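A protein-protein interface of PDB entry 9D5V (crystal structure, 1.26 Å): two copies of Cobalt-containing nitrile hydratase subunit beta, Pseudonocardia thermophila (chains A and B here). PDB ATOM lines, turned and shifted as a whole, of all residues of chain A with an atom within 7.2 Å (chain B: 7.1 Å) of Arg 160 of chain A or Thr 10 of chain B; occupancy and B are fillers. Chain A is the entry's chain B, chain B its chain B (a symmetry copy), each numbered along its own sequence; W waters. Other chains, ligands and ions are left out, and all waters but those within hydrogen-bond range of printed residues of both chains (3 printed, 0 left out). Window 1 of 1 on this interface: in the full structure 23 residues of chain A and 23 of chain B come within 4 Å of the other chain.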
ATOM      1  N   MET A   1      20.009   6.626 -25.073  1.00  0.00           N
ATOM      2  CA  MET A   1      19.228   6.327 -26.277  1.00  0.00           C
ATOM      3  C   MET A   1      18.737   4.875 -26.238  1.00  0.00           C
ATOM      4  O   MET A   1      19.555   3.974 -26.108  1.00  0.00           O
ATOM      5  CB  MET A   1      20.140   6.527 -27.516  1.00  0.00           C
ATOM      6  CG  MET A   1      19.662   5.855 -28.835  1.00  0.00           C
ATOM      7  SD  MET A   1      18.752   6.985 -29.952  1.00  0.00           S
ATOM      8  CE  MET A   1      17.849   5.840 -30.972  1.00  0.00           C
ATOM      9  N   ASN A   2      17.422   4.636 -26.347  1.00  0.00           N
ATOM     10  CA  ASN A   2      16.893   3.282 -26.575  1.00  0.00           C
ATOM     11  C   ASN A   2      16.895   2.937 -28.070  1.00  0.00           C
ATOM     12  O   ASN A   2      15.893   2.516 -28.651  1.00  0.00           O
ATOM     13  CB  ASN A   2      15.493   3.076 -25.996  1.00  0.00           C
ATOM     14  CG  ASN A   2      15.460   3.016 -24.465  1.00  0.00           C
ATOM     15  OD1 ASN A   2      16.500   3.020 -23.802  1.00  0.00           O
ATOM     16  ND2 ASN A   2      14.246   2.911 -23.900  1.00  0.00           N
ATOM     17  N   GLY A   3      18.077   3.102 -28.699  1.00  0.00           N
ATOM     18  CA  GLY A   3      18.198   2.934 -30.132  1.00  0.00           C
ATOM     19  C   GLY A   3      18.399   1.500 -30.561  1.00  0.00           C
ATOM     20  O   GLY A   3      18.749   0.629 -29.765  1.00  0.00           O
ATOM     21  N   VAL A   4      18.172   1.271 -31.859  1.00  0.00           N
ATOM     22  CA  VAL A   4      18.323  -0.062 -32.439  1.00  0.00           C
ATOM     23  C   VAL A   4      19.768  -0.513 -32.406  1.00  0.00           C
ATOM     24  O   VAL A   4      20.039  -1.715 -32.412  1.00  0.00           O
ATOM     25  CB  VAL A   4      17.738  -0.120 -33.866  1.00  0.00           C
ATOM     26  CG1 VAL A   4      18.078  -1.436 -34.517  1.00  0.00           C
ATOM     27  CG2 VAL A   4      16.214   0.059 -33.827  1.00  0.00           C
ATOM     28  N   TYR A   5      20.712   0.433 -32.386  1.00  0.00           N
ATOM     29  CA  TYR A   5      22.132   0.102 -32.281  1.00  0.00           C
ATOM     30  C   TYR A   5      22.430  -0.726 -31.032  1.00  0.00           C
ATOM     31  O   TYR A   5      23.406  -1.485 -31.006  1.00  0.00           O
ATOM     32  CB  TYR A   5      22.934   1.399 -32.234  1.00  0.00           C
ATOM     33  CG  TYR A   5      22.815   2.066 -30.887  1.00  0.00           C
ATOM     34  CD1 TYR A   5      21.759   2.918 -30.605  1.00  0.00           C
ATOM     35  CD2 TYR A   5      23.729   1.799 -29.875  1.00  0.00           C
ATOM     36  CE1 TYR A   5      21.636   3.504 -29.361  1.00  0.00           C
ATOM     37  CE2 TYR A   5      23.613   2.373 -28.636  1.00  0.00           C
ATOM     38  CZ  TYR A   5      22.567   3.220 -28.374  1.00  0.00           C
ATOM     39  OH  TYR A   5      22.471   3.809 -27.123  1.00  0.00           O
ATOM     40  N   ASP A   6      21.631  -0.558 -29.975  1.00  0.00           N
ATOM     41  CA  ASP A   6      21.761  -1.326 -28.731  1.00  0.00           C
ATOM     42  C   ASP A   6      21.191  -2.720 -29.015  1.00  0.00           C
ATOM     43  O   ASP A   6      20.052  -3.062 -28.672  1.00  0.00           O
ATOM     44  CB  ASP A   6      21.069  -0.564 -27.597  1.00  0.00           C
ATOM     45  CG  ASP A   6      20.923  -1.364 -26.307  1.00  0.00           C
ATOM     46  OD1 ASP A   6      21.648  -2.365 -26.091  1.00  0.00           O
ATOM     47  OD2 ASP A   6      20.064  -0.952 -25.483  1.00  0.00           O
ATOM     48  N   VAL A   7      22.011  -3.534 -29.695  1.00  0.00           N
ATOM     49  CA  VAL A   7      21.553  -4.791 -30.292  1.00  0.00           C
ATOM     50  C   VAL A   7      21.799  -6.027 -29.428  1.00  0.00           C
ATOM     51  O   VAL A   7      21.342  -7.121 -29.800  1.00  0.00           O
ATOM     52  CB  VAL A   7      22.182  -5.018 -31.685  1.00  0.00           C
ATOM     53  CG1 VAL A   7      21.813  -3.895 -32.621  1.00  0.00           C
ATOM     54  CG2 VAL A   7      23.724  -5.130 -31.565  1.00  0.00           C
ATOM     55  N   GLY A   8      22.516  -5.900 -28.311  1.00  0.00           N
ATOM     56  CA  GLY A   8      22.774  -7.038 -27.447  1.00  0.00           C
ATOM     57  C   GLY A   8      21.516  -7.771 -27.053  1.00  0.00           C
ATOM     58  O   GLY A   8      20.601  -7.187 -26.468  1.00  0.00           O
ATOM     59  N   THR A  10      19.348  -9.063 -29.164  1.00  0.00           N
ATOM     60  CA  THR A  10      18.361  -9.060 -30.236  1.00  0.00           C
ATOM     61  C   THR A  10      18.448 -10.353 -31.035  1.00  0.00           C
ATOM     62  O   THR A  10      19.538 -10.867 -31.300  1.00  0.00           O
ATOM     63  CB  THR A  10      18.599  -7.864 -31.159  1.00  0.00           C
ATOM     64  OG1 THR A  10      18.368  -6.648 -30.437  1.00  0.00           O
ATOM     65  CG2 THR A  10      17.678  -7.926 -32.377  1.00  0.00           C
ATOM     66  N   PRO A  60      17.560   3.831 -38.207  1.00  0.00           N
ATOM     67  CA  PRO A  60      17.990   2.475 -37.844  1.00  0.00           C
ATOM     68  C   PRO A  60      18.091   1.525 -39.027  1.00  0.00           C
ATOM     69  O   PRO A  60      18.981   0.659 -39.031  1.00  0.00           O
ATOM     70  CB  PRO A  60      16.947   2.027 -36.798  1.00  0.00           C
ATOM     71  CG  PRO A  60      15.984   3.144 -36.646  1.00  0.00           C
ATOM     72  CD  PRO A  60      16.173   4.086 -37.797  1.00  0.00           C
ATOM     73  N   PHE A 147      21.800  -2.891 -11.649  1.00  0.00           N
ATOM     74  CA  PHE A 147      21.985  -1.906 -12.701  1.00  0.00           C
ATOM     75  C   PHE A 147      20.736  -1.055 -12.851  1.00  0.00           C
ATOM     76  O   PHE A 147      19.609  -1.556 -12.809  1.00  0.00           O
ATOM     77  CB  PHE A 147      22.302  -2.594 -14.024  1.00  0.00           C
ATOM     78  CG  PHE A 147      22.930  -1.687 -15.044  1.00  0.00           C
ATOM     79  CD1 PHE A 147      22.144  -0.819 -15.788  1.00  0.00           C
ATOM     80  CD2 PHE A 147      24.301  -1.707 -15.267  1.00  0.00           C
ATOM     81  CE1 PHE A 147      22.711   0.008 -16.745  1.00  0.00           C
ATOM     82  CE2 PHE A 147      24.882  -0.884 -16.233  1.00  0.00           C
ATOM     83  CZ  PHE A 147      24.083  -0.024 -16.972  1.00  0.00           C
ATOM     84  N   SER A 148      20.957   0.234 -13.050  1.00  0.00           N
ATOM     85  CA  SER A 148      19.890   1.222 -13.099  1.00  0.00           C
ATOM     86  C   SER A 148      18.852   0.869 -14.162  1.00  0.00           C
ATOM     87  O   SER A 148      19.166   0.306 -15.215  1.00  0.00           O
ATOM     88  CB  SER A 148      20.514   2.583 -13.421  1.00  0.00           C
ATOM     89  OG  SER A 148      19.528   3.569 -13.628  1.00  0.00           O
ATOM     90  N   SER A 151      16.278   5.324 -18.308  1.00  0.00           N
ATOM     91  CA  SER A 151      16.267   5.169 -19.762  1.00  0.00           C
ATOM     92  C   SER A 151      16.391   6.544 -20.386  1.00  0.00           C
ATOM     93  O   SER A 151      15.451   7.057 -21.009  1.00  0.00           O
ATOM     94  CB  SER A 151      14.991   4.456 -20.213  1.00  0.00           C
ATOM     95  OG  SER A 151      13.849   5.159 -19.754  1.00  0.00           O
ATOM     96  N   LYS A 153      17.146   9.692 -22.802  1.00  0.00           N
ATOM     97  CA  LYS A 153      17.061   9.811 -24.248  1.00  0.00           C
ATOM     98  C   LYS A 153      18.376  10.224 -24.878  1.00  0.00           C
ATOM     99  O   LYS A 153      18.576   9.989 -26.076  1.00  0.00           O
ATOM    100  CB  LYS A 153      15.921  10.734 -24.663  1.00  0.00           C
ATOM    101  CG  LYS A 153      14.587  10.127 -24.325  1.00  0.00           C
ATOM    102  CD  LYS A 153      13.716   9.985 -25.562  1.00  0.00           C
ATOM    103  CE  LYS A 153      12.716   8.851 -25.351  1.00  0.00           C
ATOM    104  NZ  LYS A 153      12.072   8.893 -23.980  1.00  0.00           N
ATOM    105  N   ARG A 157      25.791   4.539 -21.857  1.00  0.00           N
ATOM    106  CA  ARG A 157      26.210   3.174 -22.180  1.00  0.00           C
ATOM    107  C   ARG A 157      25.437   2.199 -21.304  1.00  0.00           C
ATOM    108  O   ARG A 157      26.023   1.434 -20.521  1.00  0.00           O
ATOM    109  CB  ARG A 157      27.721   2.986 -22.001  1.00  0.00           C
ATOM    110  CG  ARG A 157      28.553   4.012 -22.747  1.00  0.00           C
ATOM    111  CD  ARG A 157      28.441   3.831 -24.243  1.00  0.00           C
ATOM    112  NE  ARG A 157      29.359   2.809 -24.723  1.00  0.00           N
ATOM    113  CZ  ARG A 157      29.467   2.444 -25.992  1.00  0.00           C
ATOM    114  NH1 ARG A 157      28.672   2.946 -26.921  1.00  0.00           N
ATOM    115  NH2 ARG A 157      30.428   1.589 -26.345  1.00  0.00           N
ATOM    116  N   ARG A 158      24.119   2.220 -21.448  1.00  0.00           N
ATOM    117  CA  ARG A 158      23.207   1.430 -20.634  1.00  0.00           C
ATOM    118  C   ARG A 158      22.458   0.461 -21.543  1.00  0.00           C
ATOM    119  O   ARG A 158      21.269   0.645 -21.802  1.00  0.00           O
ATOM    120  CB  ARG A 158      22.227   2.361 -19.888  1.00  0.00           C
ATOM    121  CG  ARG A 158      22.890   3.419 -19.030  1.00  0.00           C
ATOM    122  CD  ARG A 158      21.892   4.516 -18.666  1.00  0.00           C
ATOM    123  NE  ARG A 158      22.481   5.504 -17.769  1.00  0.00           N
ATOM    124  CZ  ARG A 158      22.313   5.490 -16.453  1.00  0.00           C
ATOM    125  NH1 ARG A 158      21.600   4.544 -15.862  1.00  0.00           N
ATOM    126  NH2 ARG A 158      22.885   6.435 -15.713  1.00  0.00           N
ATOM    127  N   ALA A 159      23.150  -0.573 -22.022  1.00  0.00           N
ATOM    128  CA  ALA A 159      22.496  -1.568 -22.865  1.00  0.00           C
ATOM    129  C   ALA A 159      21.234  -2.081 -22.187  1.00  0.00           C
ATOM    130  O   ALA A 159      21.226  -2.365 -20.983  1.00  0.00           O
ATOM    131  CB  ALA A 159      23.442  -2.740 -23.124  1.00  0.00           C
ATOM    132  N   ARG A 160      20.168  -2.237 -22.975  1.00  0.00           N
ATOM    133  CA  ARG A 160      18.878  -2.575 -22.383  1.00  0.00           C
ATOM    134  C   ARG A 160      18.904  -3.945 -21.708  1.00  0.00           C
ATOM    135  O   ARG A 160      18.215  -4.153 -20.701  1.00  0.00           O
ATOM    136  CB  ARG A 160      17.805  -2.527 -23.452  1.00  0.00           C
ATOM    137  CG  ARG A 160      17.166  -1.150 -23.603  1.00  0.00           C
ATOM    138  CD  ARG A 160      16.172  -1.250 -24.757  1.00  0.00           C
ATOM    139  NE  ARG A 160      16.863  -1.396 -26.038  1.00  0.00           N
ATOM    140  CZ  ARG A 160      16.268  -1.320 -27.226  1.00  0.00           C
ATOM    141  NH1 ARG A 160      14.950  -1.149 -27.331  1.00  0.00           N
ATOM    142  NH2 ARG A 160      17.002  -1.475 -28.332  1.00  0.00           N
ATOM    143  N   TYR A 161      19.722  -4.877 -22.218  1.00  0.00           N
ATOM    144  CA  TYR A 161      19.756  -6.229 -21.671  1.00  0.00           C
ATOM    145  C   TYR A 161      20.321  -6.311 -20.257  1.00  0.00           C
ATOM    146  O   TYR A 161      20.117  -7.339 -19.602  1.00  0.00           O
ATOM    147  CB  TYR A 161      20.459  -7.210 -22.630  1.00  0.00           C
ATOM    148  CG  TYR A 161      21.984  -7.226 -22.589  1.00  0.00           C
ATOM    149  CD1 TYR A 161      22.738  -6.364 -23.381  1.00  0.00           C
ATOM    150  CD2 TYR A 161      22.674  -8.140 -21.799  1.00  0.00           C
ATOM    151  CE1 TYR A 161      24.134  -6.385 -23.364  1.00  0.00           C
ATOM    152  CE2 TYR A 161      24.079  -8.163 -21.775  1.00  0.00           C
ATOM    153  CZ  TYR A 161      24.798  -7.292 -22.564  1.00  0.00           C
ATOM    154  OH  TYR A 161      26.185  -7.340 -22.540  1.00  0.00           O
ATOM    155  N   VAL A 162      21.003  -5.265 -19.766  1.00  0.00           N
ATOM    156  CA  VAL A 162      21.549  -5.274 -18.406  1.00  0.00           C
ATOM    157  C   VAL A 162      20.734  -4.434 -17.418  1.00  0.00           C
ATOM    158  O   VAL A 162      20.986  -4.505 -16.200  1.00  0.00           O
ATOM    159  CB  VAL A 162      23.052  -4.896 -18.369  1.00  0.00           C
ATOM    160  CG1 VAL A 162      23.887  -5.896 -19.168  1.00  0.00           C
ATOM    161  CG2 VAL A 162      23.284  -3.476 -18.851  1.00  0.00           C
ATOM    162  N   ARG A 163      19.763  -3.658 -17.894  1.00  0.00           N
ATOM    163  CA  ARG A 163      19.048  -2.753 -17.009  1.00  0.00           C
ATOM    164  C   ARG A 163      18.201  -3.516 -15.999  1.00  0.00           C
ATOM    165  O   ARG A 163      17.509  -4.481 -16.338  1.00  0.00           O
ATOM    166  CB  ARG A 163      18.174  -1.816 -17.825  1.00  0.00           C
ATOM    167  CG  ARG A 163      18.970  -0.903 -18.730  1.00  0.00           C
ATOM    168  CD  ARG A 163      18.055   0.123 -19.391  1.00  0.00           C
ATOM    169  NE  ARG A 163      18.709   0.746 -20.530  1.00  0.00           N
ATOM    170  CZ  ARG A 163      18.105   1.555 -21.388  1.00  0.00           C
ATOM    171  NH1 ARG A 163      16.822   1.862 -21.259  1.00  0.00           N
ATOM    172  NH2 ARG A 163      18.808   2.072 -22.397  1.00  0.00           N
ATOM    173  N   GLY A 164      18.248  -3.050 -14.747  1.00  0.00           N
ATOM    174  CA  GLY A 164      17.527  -3.666 -13.654  1.00  0.00           C
ATOM    175  C   GLY A 164      18.074  -4.998 -13.204  1.00  0.00           C
ATOM    176  O   GLY A 164      17.472  -5.629 -12.327  1.00  0.00           O
ATOM    177  N   LYS A 165      19.201  -5.442 -13.761  1.00  0.00           N
ATOM    178  CA  LYS A 165      19.786  -6.739 -13.448  1.00  0.00           C
ATOM    179  C   LYS A 165      20.803  -6.640 -12.303  1.00  0.00           C
ATOM    180  O   LYS A 165      21.390  -5.588 -12.039  1.00  0.00           O
ATOM    181  CB  LYS A 165      20.451  -7.310 -14.695  1.00  0.00           C
ATOM    182  CG  LYS A 165      19.489  -7.501 -15.840  1.00  0.00           C
ATOM    183  CD  LYS A 165      18.469  -8.548 -15.496  1.00  0.00           C
ATOM    184  CE  LYS A 165      17.598  -8.864 -16.676  1.00  0.00           C
ATOM    185  NZ  LYS A 165      16.665  -9.960 -16.351  1.00  0.00           N
ATOM    186  N   TYR A 216      30.341  -6.642 -17.904  1.00  0.00           N
ATOM    187  CA  TYR A 216      29.875  -5.387 -18.462  1.00  0.00           C
ATOM    188  C   TYR A 216      30.434  -4.249 -17.630  1.00  0.00           C
ATOM    189  O   TYR A 216      30.463  -4.333 -16.404  1.00  0.00           O
ATOM    190  CB  TYR A 216      28.349  -5.350 -18.444  1.00  0.00           C
ATOM    191  CG  TYR A 216      27.724  -4.188 -19.202  1.00  0.00           C
ATOM    192  CD1 TYR A 216      27.583  -2.942 -18.604  1.00  0.00           C
ATOM    193  CD2 TYR A 216      27.243  -4.354 -20.503  1.00  0.00           C
ATOM    194  CE1 TYR A 216      26.999  -1.893 -19.274  1.00  0.00           C
ATOM    195  CE2 TYR A 216      26.653  -3.311 -21.186  1.00  0.00           C
ATOM    196  CZ  TYR A 216      26.534  -2.079 -20.561  1.00  0.00           C
ATOM    197  OH  TYR A 216      25.960  -1.017 -21.238  1.00  0.00           O
ATOM    198  N   VAL B   4      13.463  -7.125 -33.677  1.00  0.00           N
ATOM    199  CA  VAL B   4      13.364  -5.671 -33.791  1.00  0.00           C
ATOM    200  C   VAL B   4      11.919  -5.221 -33.822  1.00  0.00           C
ATOM    201  O   VAL B   4      11.621  -4.081 -33.464  1.00  0.00           O
ATOM    202  CB  VAL B   4      14.151  -5.153 -35.014  1.00  0.00           C
ATOM    203  CG1 VAL B   4      13.877  -3.686 -35.228  1.00  0.00           C
ATOM    204  CG2 VAL B   4      15.657  -5.373 -34.813  1.00  0.00           C
ATOM    205  N   ASP B   6       9.720  -5.948 -31.817  1.00  0.00           N
ATOM    206  CA  ASP B   6       9.389  -5.639 -30.421  1.00  0.00           C
ATOM    207  C   ASP B   6       9.959  -4.246 -30.134  1.00  0.00           C
ATOM    208  O   ASP B   6      11.026  -4.068 -29.532  1.00  0.00           O
ATOM    209  CB  ASP B   6       9.926  -6.755 -29.521  1.00  0.00           C
ATOM    210  CG  ASP B   6       9.861  -6.438 -28.030  1.00  0.00           C
ATOM    211  OD1 ASP B   6       9.087  -5.550 -27.600  1.00  0.00           O
ATOM    212  OD2 ASP B   6      10.600  -7.125 -27.275  1.00  0.00           O
ATOM    213  N   VAL B   7       9.227  -3.229 -30.614  1.00  0.00           N
ATOM    214  CA  VAL B   7       9.735  -1.857 -30.679  1.00  0.00           C
ATOM    215  C   VAL B   7       9.334  -0.977 -29.497  1.00  0.00           C
ATOM    216  O   VAL B   7       9.813   0.166 -29.408  1.00  0.00           O
ATOM    217  CB  VAL B   7       9.312  -1.160 -31.992  1.00  0.00           C
ATOM    218  CG1 VAL B   7       9.842  -1.913 -33.185  1.00  0.00           C
ATOM    219  CG2 VAL B   7       7.767  -1.056 -32.068  1.00  0.00           C
ATOM    220  N   GLY B   8       8.464  -1.453 -28.605  1.00  0.00           N
ATOM    221  CA  GLY B   8       8.053  -0.666 -27.457  1.00  0.00           C
ATOM    222  C   GLY B   8       9.220  -0.140 -26.660  1.00  0.00           C
ATOM    223  O   GLY B   8      10.055  -0.910 -26.177  1.00  0.00           O
ATOM    224  N   GLY B   9       9.288   1.182 -26.518  1.00  0.00           N
ATOM    225  CA  GLY B   9      10.355   1.834 -25.794  1.00  0.00           C
ATOM    226  C   GLY B   9      11.570   2.184 -26.622  1.00  0.00           C
ATOM    227  O   GLY B   9      12.462   2.873 -26.117  1.00  0.00           O
ATOM    228  N   THR B  10      11.641   1.730 -27.872  1.00  0.00           N
ATOM    229  CA  THR B  10      12.775   2.062 -28.725  1.00  0.00           C
ATOM    230  C   THR B  10      12.773   3.550 -29.048  1.00  0.00           C
ATOM    231  O   THR B  10      11.721   4.151 -29.281  1.00  0.00           O
ATOM    232  CB  THR B  10      12.705   1.252 -30.021  1.00  0.00           C
ATOM    233  OG1 THR B  10      12.859  -0.141 -29.724  1.00  0.00           O
ATOM    234  CG2 THR B  10      13.793   1.696 -30.999  1.00  0.00           C
ATOM    235  N   ASP B  11      13.953   4.146 -29.053  1.00  0.00           N
ATOM    236  CA  ASP B  11      14.114   5.539 -29.428  1.00  0.00           C
ATOM    237  C   ASP B  11      14.676   5.630 -30.846  1.00  0.00           C
ATOM    238  O   ASP B  11      15.239   4.674 -31.384  1.00  0.00           O
ATOM    239  CB  ASP B  11      15.072   6.253 -28.465  1.00  0.00           C
ATOM    240  CG  ASP B  11      14.510   6.397 -27.062  1.00  0.00           C
ATOM    241  OD1 ASP B  11      13.286   6.606 -26.929  1.00  0.00           O
ATOM    242  OD2 ASP B  11      15.295   6.334 -26.088  1.00  0.00           O
ATOM    243  N   GLY B  12      14.526   6.811 -31.444  1.00  0.00           N
ATOM    244  CA  GLY B  12      15.193   7.118 -32.696  1.00  0.00           C
ATOM    245  C   GLY B  12      14.524   6.609 -33.949  1.00  0.00           C
ATOM    246  O   GLY B  12      15.179   6.544 -34.995  1.00  0.00           O
ATOM    247  N   LEU B  13      13.237   6.261 -33.892  1.00  0.00           N
ATOM    248  CA  LEU B  13      12.565   5.657 -35.038  1.00  0.00           C
ATOM    249  C   LEU B  13      11.974   6.686 -36.009  1.00  0.00           C
ATOM    250  O   LEU B  13      11.650   6.332 -37.152  1.00  0.00           O
ATOM    251  CB  LEU B  13      11.491   4.678 -34.550  1.00  0.00           C
ATOM    252  CG  LEU B  13      12.060   3.269 -34.323  1.00  0.00           C
ATOM    253  CD1 LEU B  13      11.055   2.339 -33.635  1.00  0.00           C
ATOM    254  CD2 LEU B  13      12.588   2.626 -35.609  1.00  0.00           C
ATOM    255  N   ARG B 160      10.097  -6.755 -24.526  1.00  0.00           N
ATOM    256  CA  ARG B 160      11.277  -6.668 -23.673  1.00  0.00           C
ATOM    257  C   ARG B 160      11.117  -5.604 -22.589  1.00  0.00           C
ATOM    258  O   ARG B 160      11.645  -5.764 -21.480  1.00  0.00           O
ATOM    259  CB  ARG B 160      12.496  -6.381 -24.526  1.00  0.00           C
ATOM    260  CG  ARG B 160      13.185  -7.644 -25.036  1.00  0.00           C
ATOM    261  CD  ARG B 160      14.335  -7.188 -25.930  1.00  0.00           C
ATOM    262  NE  ARG B 160      13.836  -6.603 -27.174  1.00  0.00           N
ATOM    263  CZ  ARG B 160      14.600  -6.290 -28.217  1.00  0.00           C
ATOM    264  NH1 ARG B 160      15.923  -6.449 -28.180  1.00  0.00           N
ATOM    265  NH2 ARG B 160      14.033  -5.754 -29.303  1.00  0.00           N
ATOM    266  N   TYR B 161      10.359  -4.535 -22.871  1.00  0.00           N
ATOM    267  CA  TYR B 161      10.211  -3.444 -21.912  1.00  0.00           C
ATOM    268  C   TYR B 161       9.442  -3.828 -20.651  1.00  0.00           C
ATOM    269  O   TYR B 161       9.522  -3.084 -19.667  1.00  0.00           O
ATOM    270  CB  TYR B 161       9.631  -2.181 -22.578  1.00  0.00           C
ATOM    271  CG  TYR B 161       8.117  -2.140 -22.758  1.00  0.00           C
ATOM    272  CD1 TYR B 161       7.510  -2.667 -23.895  1.00  0.00           C
ATOM    273  CD2 TYR B 161       7.295  -1.527 -21.818  1.00  0.00           C
ATOM    274  CE1 TYR B 161       6.125  -2.617 -24.077  1.00  0.00           C
ATOM    275  CE2 TYR B 161       5.903  -1.478 -21.993  1.00  0.00           C
ATOM    276  CZ  TYR B 161       5.329  -2.015 -23.125  1.00  0.00           C
ATOM    277  OH  TYR B 161       3.954  -1.943 -23.291  1.00  0.00           O
ATOM    278  N   TRP B 204      10.351   2.897 -16.968  1.00  0.00           N
ATOM    279  CA  TRP B 204      11.370   3.736 -17.587  1.00  0.00           C
ATOM    280  C   TRP B 204      12.315   4.390 -16.592  1.00  0.00           C
ATOM    281  O   TRP B 204      13.182   5.169 -17.007  1.00  0.00           O
ATOM    282  CB  TRP B 204      10.724   4.803 -18.498  1.00  0.00           C
ATOM    283  CG  TRP B 204       9.608   4.240 -19.336  1.00  0.00           C
ATOM    284  CD1 TRP B 204       8.286   4.552 -19.254  1.00  0.00           C
ATOM    285  CD2 TRP B 204       9.721   3.245 -20.362  1.00  0.00           C
ATOM    286  NE1 TRP B 204       7.564   3.809 -20.155  1.00  0.00           N
ATOM    287  CE2 TRP B 204       8.423   3.003 -20.853  1.00  0.00           C
ATOM    288  CE3 TRP B 204      10.794   2.534 -20.911  1.00  0.00           C
ATOM    289  CZ2 TRP B 204       8.166   2.082 -21.870  1.00  0.00           C
ATOM    290  CZ3 TRP B 204      10.538   1.615 -21.915  1.00  0.00           C
ATOM    291  CH2 TRP B 204       9.234   1.400 -22.386  1.00  0.00           C
HETATM  292  O   HOH W   1      17.925  -8.107 -25.869  1.00  0.00           O
HETATM  293  O   HOH W   2      16.912   3.509 -33.423  1.00  0.00           O
HETATM  294  O   HOH W   3      12.590  -0.313 -24.918  1.00  0.00           O
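Water W2 bridges O of Asp 11 of chain B (2.9 Å) and N of Val 4 of chain A (3.0 Å). Water W3 lies within hydrogen-bond range of O of Gly 8 of chain B (2.9 Å), O of Gly 9 of chain B (3.4 Å) and NH1 of Arg 160 of chain A (3.5 Å). Water W1 lies within hydrogen-bond range of the backbone carbonyl oxygen (O) of Gly 8 of chain A and the guanidinium group (NH1) of Arg 160 of chain B.
Printed residues of chain A that touch a printed residue of chain B: Met 1, Asn 2, Gly 3, Thr 10, Pro 60, Ser 151, Lys 153 and Arg 160. Hydrophobic or aromatic side chains of chain A within 4 Å of the printed part of chain B: Met 1 and Pro 60. Among the printed residues, 12 pairs touch across the chains.
The side-chain amide nitrogen of Asn 2 of chain A lies within hydrogen-bond range of the backbone carbonyl oxygen of Gly 9 of chain B (2.8 Å). The backbone carbonyl oxygen of Asn 2 of chain A sits at hydrogen-bond distance from the backbone NH of Asp 11 of chain B, at 2.6 Å. OG1 of Thr 10 of chain A is in hydrogen-bond range of NH1 of Arg 160 of chain B (3.3 Å). OG of Ser 151 of chain A is in hydrogen-bond range of O of Trp 204 of chain B (2.8 Å). The side-chain amino group (NZ) of Lys 153 of chain A lies within salt-bridge range of the side-chain carboxylate (OD1) of Asp 11 of chain B (3.9 Å). NH1 of Arg 160 of chain A lies within hydrogen-bond range of OG1 of Thr 10 of chain B, 3.3 Å away.
Thr 10 of chain A touches Arg 160 of chain B, and with the chains exchanged Arg 160 of chain A touches Thr 10 of chain B. 7 positions are printed for both chains.
Among the printed residues, pairs that only touch across the chains: Met 1 of chain A with Asp 11 of chain B (2.9 Å), Met 1 of chain A with Gly 12 of chain B (3.4 Å), Asn 2 of chain A with Thr 10 of chain B (3.2 Å), Gly 3 of chain A with Asp 11 of chain B (3.7 Å), Pro 60 of chain A with Gly 12 of chain B (3.9 Å) and Pro 60 of chain A with Leu 13 of chain B (3.6 Å).
The backbone carbonyl oxygen of Met 1 of chain A lies within hydrogen-bond range of the side-chain hydroxyl of Tyr 5 of chain A, at 3.1 Å. NH1 of Arg 163 of chain A is in hydrogen-bond range of OD1 of Asn 2 of chain A. The backbone carbonyl oxygen (O) of Gly 3 of chain A lies within hydrogen-bond range of the guanidinium group (NH2) of Arg 160 of chain A (3.1 Å). The guanidinium group (NE) of Arg 160 of chain A lies within salt-bridge range of the side-chain carboxylate (OD2) of Asp 6 of chain A (3.3 Å). O of Val 7 of chain A is in hydrogen-bond range of OG1 of Thr 10 of chain A (3.1 Å). The guanidinium group (NE) of Arg 160 of chain B lies within salt-bridge range of the side-chain carboxylate (OD2) of Asp 6 of chain B (3.3 Å).
Arg 160 of chain A touches just one residue of chain B: Thr 10 (3.3 Å). Gly 9 of chain B touches one residue of chain A. Printed residues of chain B within 4 Å of Pro 60 of chain A: Gly 12 (3.9 Å) and Leu 13 (3.6 Å). Printed residues of chain A within 4 Å of Gly 12 of chain B: Met 1 (3.4 Å) and Pro 60 (3.9 Å). The nearest residue of chain B that does not touch Arg 160 of chain A is Gly 9 of chain B (4.8 Å). The nearest residue of chain A that does not touch Thr 10 of chain B is Val 4 of chain A (4.1 Å).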
